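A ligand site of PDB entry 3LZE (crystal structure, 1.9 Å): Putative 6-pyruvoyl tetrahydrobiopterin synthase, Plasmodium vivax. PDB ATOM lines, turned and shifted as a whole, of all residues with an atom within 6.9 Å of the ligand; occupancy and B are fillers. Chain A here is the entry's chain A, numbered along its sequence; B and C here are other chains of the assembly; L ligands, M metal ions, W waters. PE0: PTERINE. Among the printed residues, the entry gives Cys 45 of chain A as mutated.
A nitrogen (N6) of the ligand lies within hydrogen-bond range of the backbone carbonyl oxygen (O) of Ile 69 of chain B (2.8 Å). An oxygen (O4) of the ligand is in hydrogen-bond range of the backbone NH (N) of Thr 134 (3.0 Å). An oxygen (O4) of the ligand sits at hydrogen-bond distance from the side-chain hydroxyl (OG1) of Thr 134. OE1 of Glu 135 sits at hydrogen-bond distance from N2 of the ligand, 3.0 Å away. OE1 of Glu 168 sits close to N4 of the ligand, 3.2 Å away. N of Phe 71 of chain B is in hydrogen-bond range of N1 of the ligand, at 3.1 Å. OH of Tyr 67 of chain B is in hydrogen-bond range of N4 of the ligand (3.5 Å).
The side-chain carboxylate (OD1) of Asp 70 of chain B sits at hydrogen-bond distance from the side-chain hydroxyl (OG) of Ser 72 of chain B. OG1 of Thr 134 sits at hydrogen-bond distance from OE1 of Glu 168 (2.8 Å). The side-chain carboxylate (OE2) of Glu 135 sits at hydrogen-bond distance from the backbone NH (N) of Val 68 of chain B (2.8 Å). NE2 of Gln 172 lies within hydrogen-bond range of OE2 of Glu 168 (2.7 Å). O of Glu 168 lies within hydrogen-bond range of ND1 of His 50 (3.2 Å). O of Gly 66 of chain B sits at hydrogen-bond distance from OG of Ser 133 (2.7 Å).
The side-chain carboxylate (OD1) of Asp 70 of chain B lies close to a nitrogen (N3) of the ligand (2.9 Å). Ser 133 touches the ligand (CA to O4, 3.5 Å). CD1 of Leu 23 of chain B touches N6 of the ligand, 3.9 Å away. Within 4 Å of the ligand: Ser 133, Thr 134, Glu 135, Glu 168, Leu 23 of chain B, Tyr 67 of chain B, Ile 69 of chain B, Asp 70 of chain B and Phe 71 of chain B. The nearest printed residue that does not touch the ligand is Ile 38 (4.3 Å).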
ATOM      1  N   HIS A  36      20.689 -14.417 -27.119  1.00  0.00           N
ATOM      2  CA  HIS A  36      21.168 -13.987 -25.790  1.00  0.00           C
ATOM      3  C   HIS A  36      21.698 -15.232 -25.083  1.00  0.00           C
ATOM      4  O   HIS A  36      21.641 -16.341 -25.634  1.00  0.00           O
ATOM      5  CB  HIS A  36      20.074 -13.354 -24.989  1.00  0.00           C
ATOM      6  CG  HIS A  36      19.199 -14.331 -24.274  1.00  0.00           C
ATOM      7  ND1 HIS A  36      18.967 -14.246 -22.925  1.00  0.00           N
ATOM      8  CD2 HIS A  36      18.517 -15.429 -24.697  1.00  0.00           C
ATOM      9  CE1 HIS A  36      18.168 -15.236 -22.542  1.00  0.00           C
ATOM     10  NE2 HIS A  36      17.872 -15.952 -23.608  1.00  0.00           N
ATOM     11  N   ILE A  38      22.042 -16.535 -20.756  1.00  0.00           N
ATOM     12  CA  ILE A  38      21.915 -16.221 -19.334  1.00  0.00           C
ATOM     13  C   ILE A  38      23.198 -16.568 -18.631  1.00  0.00           C
ATOM     14  O   ILE A  38      23.726 -17.652 -18.837  1.00  0.00           O
ATOM     15  CB  ILE A  38      20.773 -17.041 -18.685  1.00  0.00           C
ATOM     16  CG1 ILE A  38      19.424 -16.657 -19.295  1.00  0.00           C
ATOM     17  CG2 ILE A  38      20.738 -16.855 -17.153  1.00  0.00           C
ATOM     18  CD1 ILE A  38      19.062 -15.183 -19.118  1.00  0.00           C
ATOM     19  N   CYS A  45      24.264 -20.330 -19.279  1.00  0.00           N
ATOM     20  CA  CYS A  45      23.624 -21.179 -20.300  1.00  0.00           C
ATOM     21  C   CYS A  45      24.329 -20.946 -21.628  1.00  0.00           C
ATOM     22  O   CYS A  45      25.161 -20.037 -21.778  1.00  0.00           O
ATOM     23  CB  CYS A  45      22.130 -20.884 -20.467  1.00  0.00           C
ATOM     24  SG  CYS A  45      21.739 -19.629 -21.745  1.00  0.00           S
ATOM     25  N   HIS A  48      21.683 -19.003 -27.467  1.00  0.00           N
ATOM     26  CA  HIS A  48      20.434 -19.415 -28.085  1.00  0.00           C
ATOM     27  C   HIS A  48      19.688 -18.143 -28.415  1.00  0.00           C
ATOM     28  O   HIS A  48      20.302 -17.081 -28.461  1.00  0.00           O
ATOM     29  CB  HIS A  48      19.646 -20.321 -27.137  1.00  0.00           C
ATOM     30  CG  HIS A  48      19.180 -19.677 -25.849  1.00  0.00           C
ATOM     31  ND1 HIS A  48      19.967 -19.631 -24.710  1.00  0.00           N
ATOM     32  CD2 HIS A  48      17.973 -19.193 -25.494  1.00  0.00           C
ATOM     33  CE1 HIS A  48      19.281 -19.066 -23.739  1.00  0.00           C
ATOM     34  NE2 HIS A  48      18.070 -18.788 -24.179  1.00  0.00           N
ATOM     35  N   HIS A  50      15.402 -16.206 -29.122  1.00  0.00           N
ATOM     36  CA  HIS A  50      13.961 -16.136 -28.904  1.00  0.00           C
ATOM     37  C   HIS A  50      13.307 -15.106 -29.789  1.00  0.00           C
ATOM     38  O   HIS A  50      13.935 -14.091 -30.160  1.00  0.00           O
ATOM     39  CB  HIS A  50      13.642 -15.696 -27.490  1.00  0.00           C
ATOM     40  CG  HIS A  50      14.169 -16.577 -26.422  1.00  0.00           C
ATOM     41  ND1 HIS A  50      13.707 -17.869 -26.210  1.00  0.00           N
ATOM     42  CD2 HIS A  50      15.118 -16.352 -25.485  1.00  0.00           C
ATOM     43  CE1 HIS A  50      14.369 -18.401 -25.193  1.00  0.00           C
ATOM     44  NE2 HIS A  50      15.232 -17.505 -24.751  1.00  0.00           N
ATOM     45  N   TYR A  52      11.009 -12.650 -28.981  1.00  0.00           N
ATOM     46  CA  TYR A  52      10.414 -11.983 -27.846  1.00  0.00           C
ATOM     47  C   TYR A  52       9.200 -11.254 -28.338  1.00  0.00           C
ATOM     48  O   TYR A  52       9.197 -10.737 -29.467  1.00  0.00           O
ATOM     49  CB  TYR A  52      11.394 -10.993 -27.219  1.00  0.00           C
ATOM     50  CG  TYR A  52      12.581 -11.597 -26.511  1.00  0.00           C
ATOM     51  CD1 TYR A  52      12.553 -11.833 -25.148  1.00  0.00           C
ATOM     52  CD2 TYR A  52      13.776 -11.869 -27.194  1.00  0.00           C
ATOM     53  CE1 TYR A  52      13.675 -12.316 -24.485  1.00  0.00           C
ATOM     54  CE2 TYR A  52      14.897 -12.347 -26.522  1.00  0.00           C
ATOM     55  CZ  TYR A  52      14.835 -12.572 -25.167  1.00  0.00           C
ATOM     56  OH  TYR A  52      15.954 -13.062 -24.488  1.00  0.00           O
ATOM     57  N   SER A 132      20.240 -10.526 -19.244  1.00  0.00           N
ATOM     58  CA  SER A 132      19.298 -10.551 -20.333  1.00  0.00           C
ATOM     59  C   SER A 132      18.099 -11.458 -20.000  1.00  0.00           C
ATOM     60  O   SER A 132      17.656 -12.264 -20.837  1.00  0.00           O
ATOM     61  CB  SER A 132      19.999 -10.994 -21.644  1.00  0.00           C
ATOM     62  OG  SER A 132      20.569 -12.287 -21.535  1.00  0.00           O
ATOM     63  N   SER A 133      17.575 -11.315 -18.785  1.00  0.00           N
ATOM     64  CA  SER A 133      16.346 -11.978 -18.384  1.00  0.00           C
ATOM     65  C   SER A 133      15.124 -11.210 -18.831  1.00  0.00           C
ATOM     66  O   SER A 133      15.153  -9.992 -19.041  1.00  0.00           O
ATOM     67  CB  SER A 133      16.295 -12.099 -16.846  1.00  0.00           C
ATOM     68  OG  SER A 133      16.182 -10.815 -16.261  1.00  0.00           O
ATOM     69  N   THR A 134      14.001 -11.923 -18.916  1.00  0.00           N
ATOM     70  CA  THR A 134      12.757 -11.333 -19.357  1.00  0.00           C
ATOM     71  C   THR A 134      12.327 -10.169 -18.484  1.00  0.00           C
ATOM     72  O   THR A 134      11.849  -9.152 -18.959  1.00  0.00           O
ATOM     73  CB  THR A 134      11.697 -12.444 -19.409  1.00  0.00           C
ATOM     74  OG1 THR A 134      12.252 -13.529 -20.171  1.00  0.00           O
ATOM     75  CG2 THR A 134      10.466 -11.988 -20.084  1.00  0.00           C
ATOM     76  N   GLU A 135      12.518 -10.326 -17.196  1.00  0.00           N
ATOM     77  CA  GLU A 135      12.193  -9.308 -16.212  1.00  0.00           C
ATOM     78  C   GLU A 135      12.966  -7.971 -16.403  1.00  0.00           C
ATOM     79  O   GLU A 135      12.370  -6.885 -16.392  1.00  0.00           O
ATOM     80  CB  GLU A 135      12.581  -9.829 -14.835  1.00  0.00           C
ATOM     81  CG  GLU A 135      11.698 -10.924 -14.283  1.00  0.00           C
ATOM     82  CD  GLU A 135      12.240 -12.326 -14.450  1.00  0.00           C
ATOM     83  OE1 GLU A 135      12.769 -12.629 -15.514  1.00  0.00           O
ATOM     84  OE2 GLU A 135      12.074 -13.161 -13.529  1.00  0.00           O
ATOM     85  N   ILE A 137      14.718  -7.063 -19.124  1.00  0.00           N
ATOM     86  CA  ILE A 137      14.392  -6.569 -20.445  1.00  0.00           C
ATOM     87  C   ILE A 137      13.040  -5.837 -20.411  1.00  0.00           C
ATOM     88  O   ILE A 137      12.918  -4.745 -20.964  1.00  0.00           O
ATOM     89  CB  ILE A 137      14.359  -7.695 -21.484  1.00  0.00           C
ATOM     90  CG1 ILE A 137      15.780  -8.213 -21.747  1.00  0.00           C
ATOM     91  CG2 ILE A 137      13.722  -7.232 -22.764  1.00  0.00           C
ATOM     92  CD1 ILE A 137      15.796  -9.613 -22.572  1.00  0.00           C
ATOM     93  N   GLU A 168       9.351 -14.380 -23.587  1.00  0.00           N
ATOM     94  CA  GLU A 168      10.488 -14.934 -24.305  1.00  0.00           C
ATOM     95  C   GLU A 168      10.058 -16.124 -25.155  1.00  0.00           C
ATOM     96  O   GLU A 168      10.761 -16.518 -26.093  1.00  0.00           O
ATOM     97  CB  GLU A 168      11.576 -15.309 -23.332  1.00  0.00           C
ATOM     98  CG  GLU A 168      11.173 -16.338 -22.310  1.00  0.00           C
ATOM     99  CD  GLU A 168      12.376 -16.907 -21.636  1.00  0.00           C
ATOM    100  OE1 GLU A 168      12.965 -16.194 -20.792  1.00  0.00           O
ATOM    101  OE2 GLU A 168      12.754 -18.055 -21.962  1.00  0.00           O
ATOM    102  N   GLN A 172       6.109 -18.215 -21.164  1.00  0.00           N
ATOM    103  CA  GLN A 172       6.870 -17.594 -20.062  1.00  0.00           C
ATOM    104  C   GLN A 172       6.928 -16.104 -20.303  1.00  0.00           C
ATOM    105  O   GLN A 172       7.580 -15.651 -21.287  1.00  0.00           O
ATOM    106  CB  GLN A 172       8.319 -18.095 -19.966  1.00  0.00           C
ATOM    107  CG  GLN A 172       8.544 -19.518 -20.374  1.00  0.00           C
ATOM    108  CD  GLN A 172       9.972 -19.992 -20.082  1.00  0.00           C
ATOM    109  OE1 GLN A 172      10.176 -21.146 -19.723  1.00  0.00           O
ATOM    110  NE2 GLN A 172      10.952 -19.105 -20.234  1.00  0.00           N
ATOM    111  N   ALA A 174       7.070 -11.988 -18.312  1.00  0.00           N
ATOM    112  CA  ALA A 174       7.250 -11.107 -17.144  1.00  0.00           C
ATOM    113  C   ALA A 174       6.567  -9.771 -17.394  1.00  0.00           C
ATOM    114  O   ALA A 174       6.641  -9.218 -18.483  1.00  0.00           O
ATOM    115  CB  ALA A 174       8.733 -10.867 -16.833  1.00  0.00           C
ATOM    116  N   LEU B  23       5.309 -12.731 -12.866  1.00  0.00           N
ATOM    117  CA  LEU B  23       5.619 -13.789 -13.825  1.00  0.00           C
ATOM    118  C   LEU B  23       4.353 -14.554 -14.133  1.00  0.00           C
ATOM    119  O   LEU B  23       3.533 -14.773 -13.248  1.00  0.00           O
ATOM    120  CB  LEU B  23       6.683 -14.727 -13.253  1.00  0.00           C
ATOM    121  CG  LEU B  23       8.065 -14.170 -12.983  1.00  0.00           C
ATOM    122  CD1 LEU B  23       9.020 -15.312 -12.595  1.00  0.00           C
ATOM    123  CD2 LEU B  23       8.587 -13.407 -14.174  1.00  0.00           C
ATOM    124  N   GLY B  66      18.756 -11.961 -11.424  1.00  0.00           N
ATOM    125  CA  GLY B  66      17.976 -11.403 -12.559  1.00  0.00           C
ATOM    126  C   GLY B  66      16.588 -12.025 -12.787  1.00  0.00           C
ATOM    127  O   GLY B  66      15.891 -11.655 -13.737  1.00  0.00           O
ATOM    128  N   TYR B  67      16.217 -12.961 -11.930  1.00  0.00           N
ATOM    129  CA  TYR B  67      14.914 -13.638 -11.976  1.00  0.00           C
ATOM    130  C   TYR B  67      14.125 -13.316 -10.711  1.00  0.00           C
ATOM    131  O   TYR B  67      14.732 -13.187  -9.658  1.00  0.00           O
ATOM    132  CB  TYR B  67      15.099 -15.143 -11.976  1.00  0.00           C
ATOM    133  CG  TYR B  67      15.805 -15.785 -13.170  1.00  0.00           C
ATOM    134  CD1 TYR B  67      15.921 -15.132 -14.381  1.00  0.00           C
ATOM    135  CD2 TYR B  67      16.312 -17.081 -13.074  1.00  0.00           C
ATOM    136  CE1 TYR B  67      16.544 -15.758 -15.471  1.00  0.00           C
ATOM    137  CE2 TYR B  67      16.931 -17.709 -14.139  1.00  0.00           C
ATOM    138  CZ  TYR B  67      17.041 -17.043 -15.346  1.00  0.00           C
ATOM    139  OH  TYR B  67      17.624 -17.653 -16.448  1.00  0.00           O
ATOM    140  N   VAL B  68      12.784 -13.249 -10.773  1.00  0.00           N
ATOM    141  CA  VAL B  68      11.963 -13.283  -9.530  1.00  0.00           C
ATOM    142  C   VAL B  68      12.092 -14.703  -8.945  1.00  0.00           C
ATOM    143  O   VAL B  68      12.451 -14.902  -7.777  1.00  0.00           O
ATOM    144  CB  VAL B  68      10.466 -12.961  -9.763  1.00  0.00           C
ATOM    145  CG1 VAL B  68       9.688 -13.070  -8.423  1.00  0.00           C
ATOM    146  CG2 VAL B  68      10.272 -11.562 -10.363  1.00  0.00           C
ATOM    147  N   ILE B  69      11.844 -15.693  -9.796  1.00  0.00           N
ATOM    148  CA  ILE B  69      12.092 -17.104  -9.520  1.00  0.00           C
ATOM    149  C   ILE B  69      12.296 -17.760 -10.909  1.00  0.00           C
ATOM    150  O   ILE B  69      11.718 -17.296 -11.914  1.00  0.00           O
ATOM    151  CB  ILE B  69      10.879 -17.720  -8.744  1.00  0.00           C
ATOM    152  CG1 ILE B  69      11.095 -19.209  -8.455  1.00  0.00           C
ATOM    153  CG2 ILE B  69       9.607 -17.566  -9.548  1.00  0.00           C
ATOM    154  CD1 ILE B  69      10.087 -19.791  -7.453  1.00  0.00           C
ATOM    155  N   ASP B  70      13.106 -18.818 -10.998  1.00  0.00           N
ATOM    156  CA  ASP B  70      13.358 -19.489 -12.315  1.00  0.00           C
ATOM    157  C   ASP B  70      12.070 -20.096 -12.929  1.00  0.00           C
ATOM    158  O   ASP B  70      11.393 -20.934 -12.281  1.00  0.00           O
ATOM    159  CB  ASP B  70      14.463 -20.561 -12.143  1.00  0.00           C
ATOM    160  CG  ASP B  70      15.016 -21.078 -13.485  1.00  0.00           C
ATOM    161  OD1 ASP B  70      14.351 -20.985 -14.553  1.00  0.00           O
ATOM    162  OD2 ASP B  70      16.159 -21.586 -13.470  1.00  0.00           O
ATOM    163  N   PHE B  71      11.730 -19.692 -14.169  1.00  0.00           N
ATOM    164  CA  PHE B  71      10.560 -20.265 -14.881  1.00  0.00           C
ATOM    165  C   PHE B  71      10.570 -21.813 -14.897  1.00  0.00           C
ATOM    166  O   PHE B  71       9.518 -22.456 -14.798  1.00  0.00           O
ATOM    167  CB  PHE B  71      10.497 -19.822 -16.347  1.00  0.00           C
ATOM    168  CG  PHE B  71      10.006 -18.409 -16.576  1.00  0.00           C
ATOM    169  CD1 PHE B  71       8.765 -18.002 -16.138  1.00  0.00           C
ATOM    170  CD2 PHE B  71      10.770 -17.522 -17.347  1.00  0.00           C
ATOM    171  CE1 PHE B  71       8.292 -16.713 -16.395  1.00  0.00           C
ATOM    172  CE2 PHE B  71      10.314 -16.233 -17.626  1.00  0.00           C
ATOM    173  CZ  PHE B  71       9.066 -15.828 -17.139  1.00  0.00           C
ATOM    174  N   SER B  72      11.748 -22.402 -15.067  1.00  0.00           N
ATOM    175  CA  SER B  72      11.877 -23.870 -15.094  1.00  0.00           C
ATOM    176  C   SER B  72      11.271 -24.579 -13.871  1.00  0.00           C
ATOM    177  O   SER B  72      10.681 -25.651 -14.021  1.00  0.00           O
ATOM    178  CB  SER B  72      13.351 -24.255 -15.250  1.00  0.00           C
ATOM    179  OG  SER B  72      14.065 -23.852 -14.105  1.00  0.00           O
ATOM    180  N   LEU B  74       8.821 -23.314 -11.854  1.00  0.00           N
ATOM    181  CA  LEU B  74       7.369 -23.147 -12.021  1.00  0.00           C
ATOM    182  C   LEU B  74       6.773 -24.178 -12.994  1.00  0.00           C
ATOM    183  O   LEU B  74       5.722 -24.797 -12.708  1.00  0.00           O
ATOM    184  CB  LEU B  74       7.004 -21.713 -12.485  1.00  0.00           C
ATOM    185  CG  LEU B  74       7.581 -20.562 -11.637  1.00  0.00           C
ATOM    186  CD1 LEU B  74       7.153 -19.181 -12.165  1.00  0.00           C
ATOM    187  CD2 LEU B  74       7.164 -20.742 -10.162  1.00  0.00           C
ATOM    188  N   HIS C  87      18.487 -24.547 -27.490  1.00  0.00           N
ATOM    189  CA  HIS C  87      19.521 -23.815 -26.743  1.00  0.00           C
ATOM    190  C   HIS C  87      20.949 -23.866 -27.353  1.00  0.00           C
ATOM    191  O   HIS C  87      21.930 -24.040 -26.646  1.00  0.00           O
ATOM    192  CB  HIS C  87      19.500 -24.232 -25.263  1.00  0.00           C
ATOM    193  CG  HIS C  87      18.533 -23.428 -24.459  1.00  0.00           C
ATOM    194  ND1 HIS C  87      18.873 -22.816 -23.277  1.00  0.00           N
ATOM    195  CD2 HIS C  87      17.251 -23.071 -24.716  1.00  0.00           C
ATOM    196  CE1 HIS C  87      17.832 -22.143 -22.809  1.00  0.00           C
ATOM    197  NE2 HIS C  87      16.825 -22.284 -23.660  1.00  0.00           N
HETATM  198  C1  PE0 L   1      14.476 -17.083 -17.803  1.00  0.00           C
HETATM  199  C4  PE0 L   1      14.086 -15.727 -17.634  1.00  0.00           C
HETATM  200  O4  PE0 L   1      14.356 -14.833 -18.469  1.00  0.00           O
HETATM  201  N2  PE0 L   1      13.365 -15.378 -16.478  1.00  0.00           N
HETATM  202  C3  PE0 L   1      13.083 -16.385 -15.489  1.00  0.00           C
HETATM  203  N6  PE0 L   1      12.404 -16.090 -14.379  1.00  0.00           N
HETATM  204  N1  PE0 L   1      13.478 -17.664 -15.682  1.00  0.00           N
HETATM  205  C2  PE0 L   1      14.166 -18.022 -16.810  1.00  0.00           C
HETATM  206  N3  PE0 L   1      14.542 -19.313 -16.974  1.00  0.00           N
HETATM  207  C6  PE0 L   1      15.228 -19.703 -18.057  1.00  0.00           C
HETATM  208  C5  PE0 L   1      15.557 -18.766 -19.035  1.00  0.00           C
HETATM  209  N4  PE0 L   1      15.197 -17.494 -18.895  1.00  0.00           N
HETATM  210 ZN    ZN M   1      16.687 -17.668 -23.301  1.00  0.00          ZN
HETATM  211  O   HOH W   1      17.393 -17.935 -21.192  1.00  0.00           O
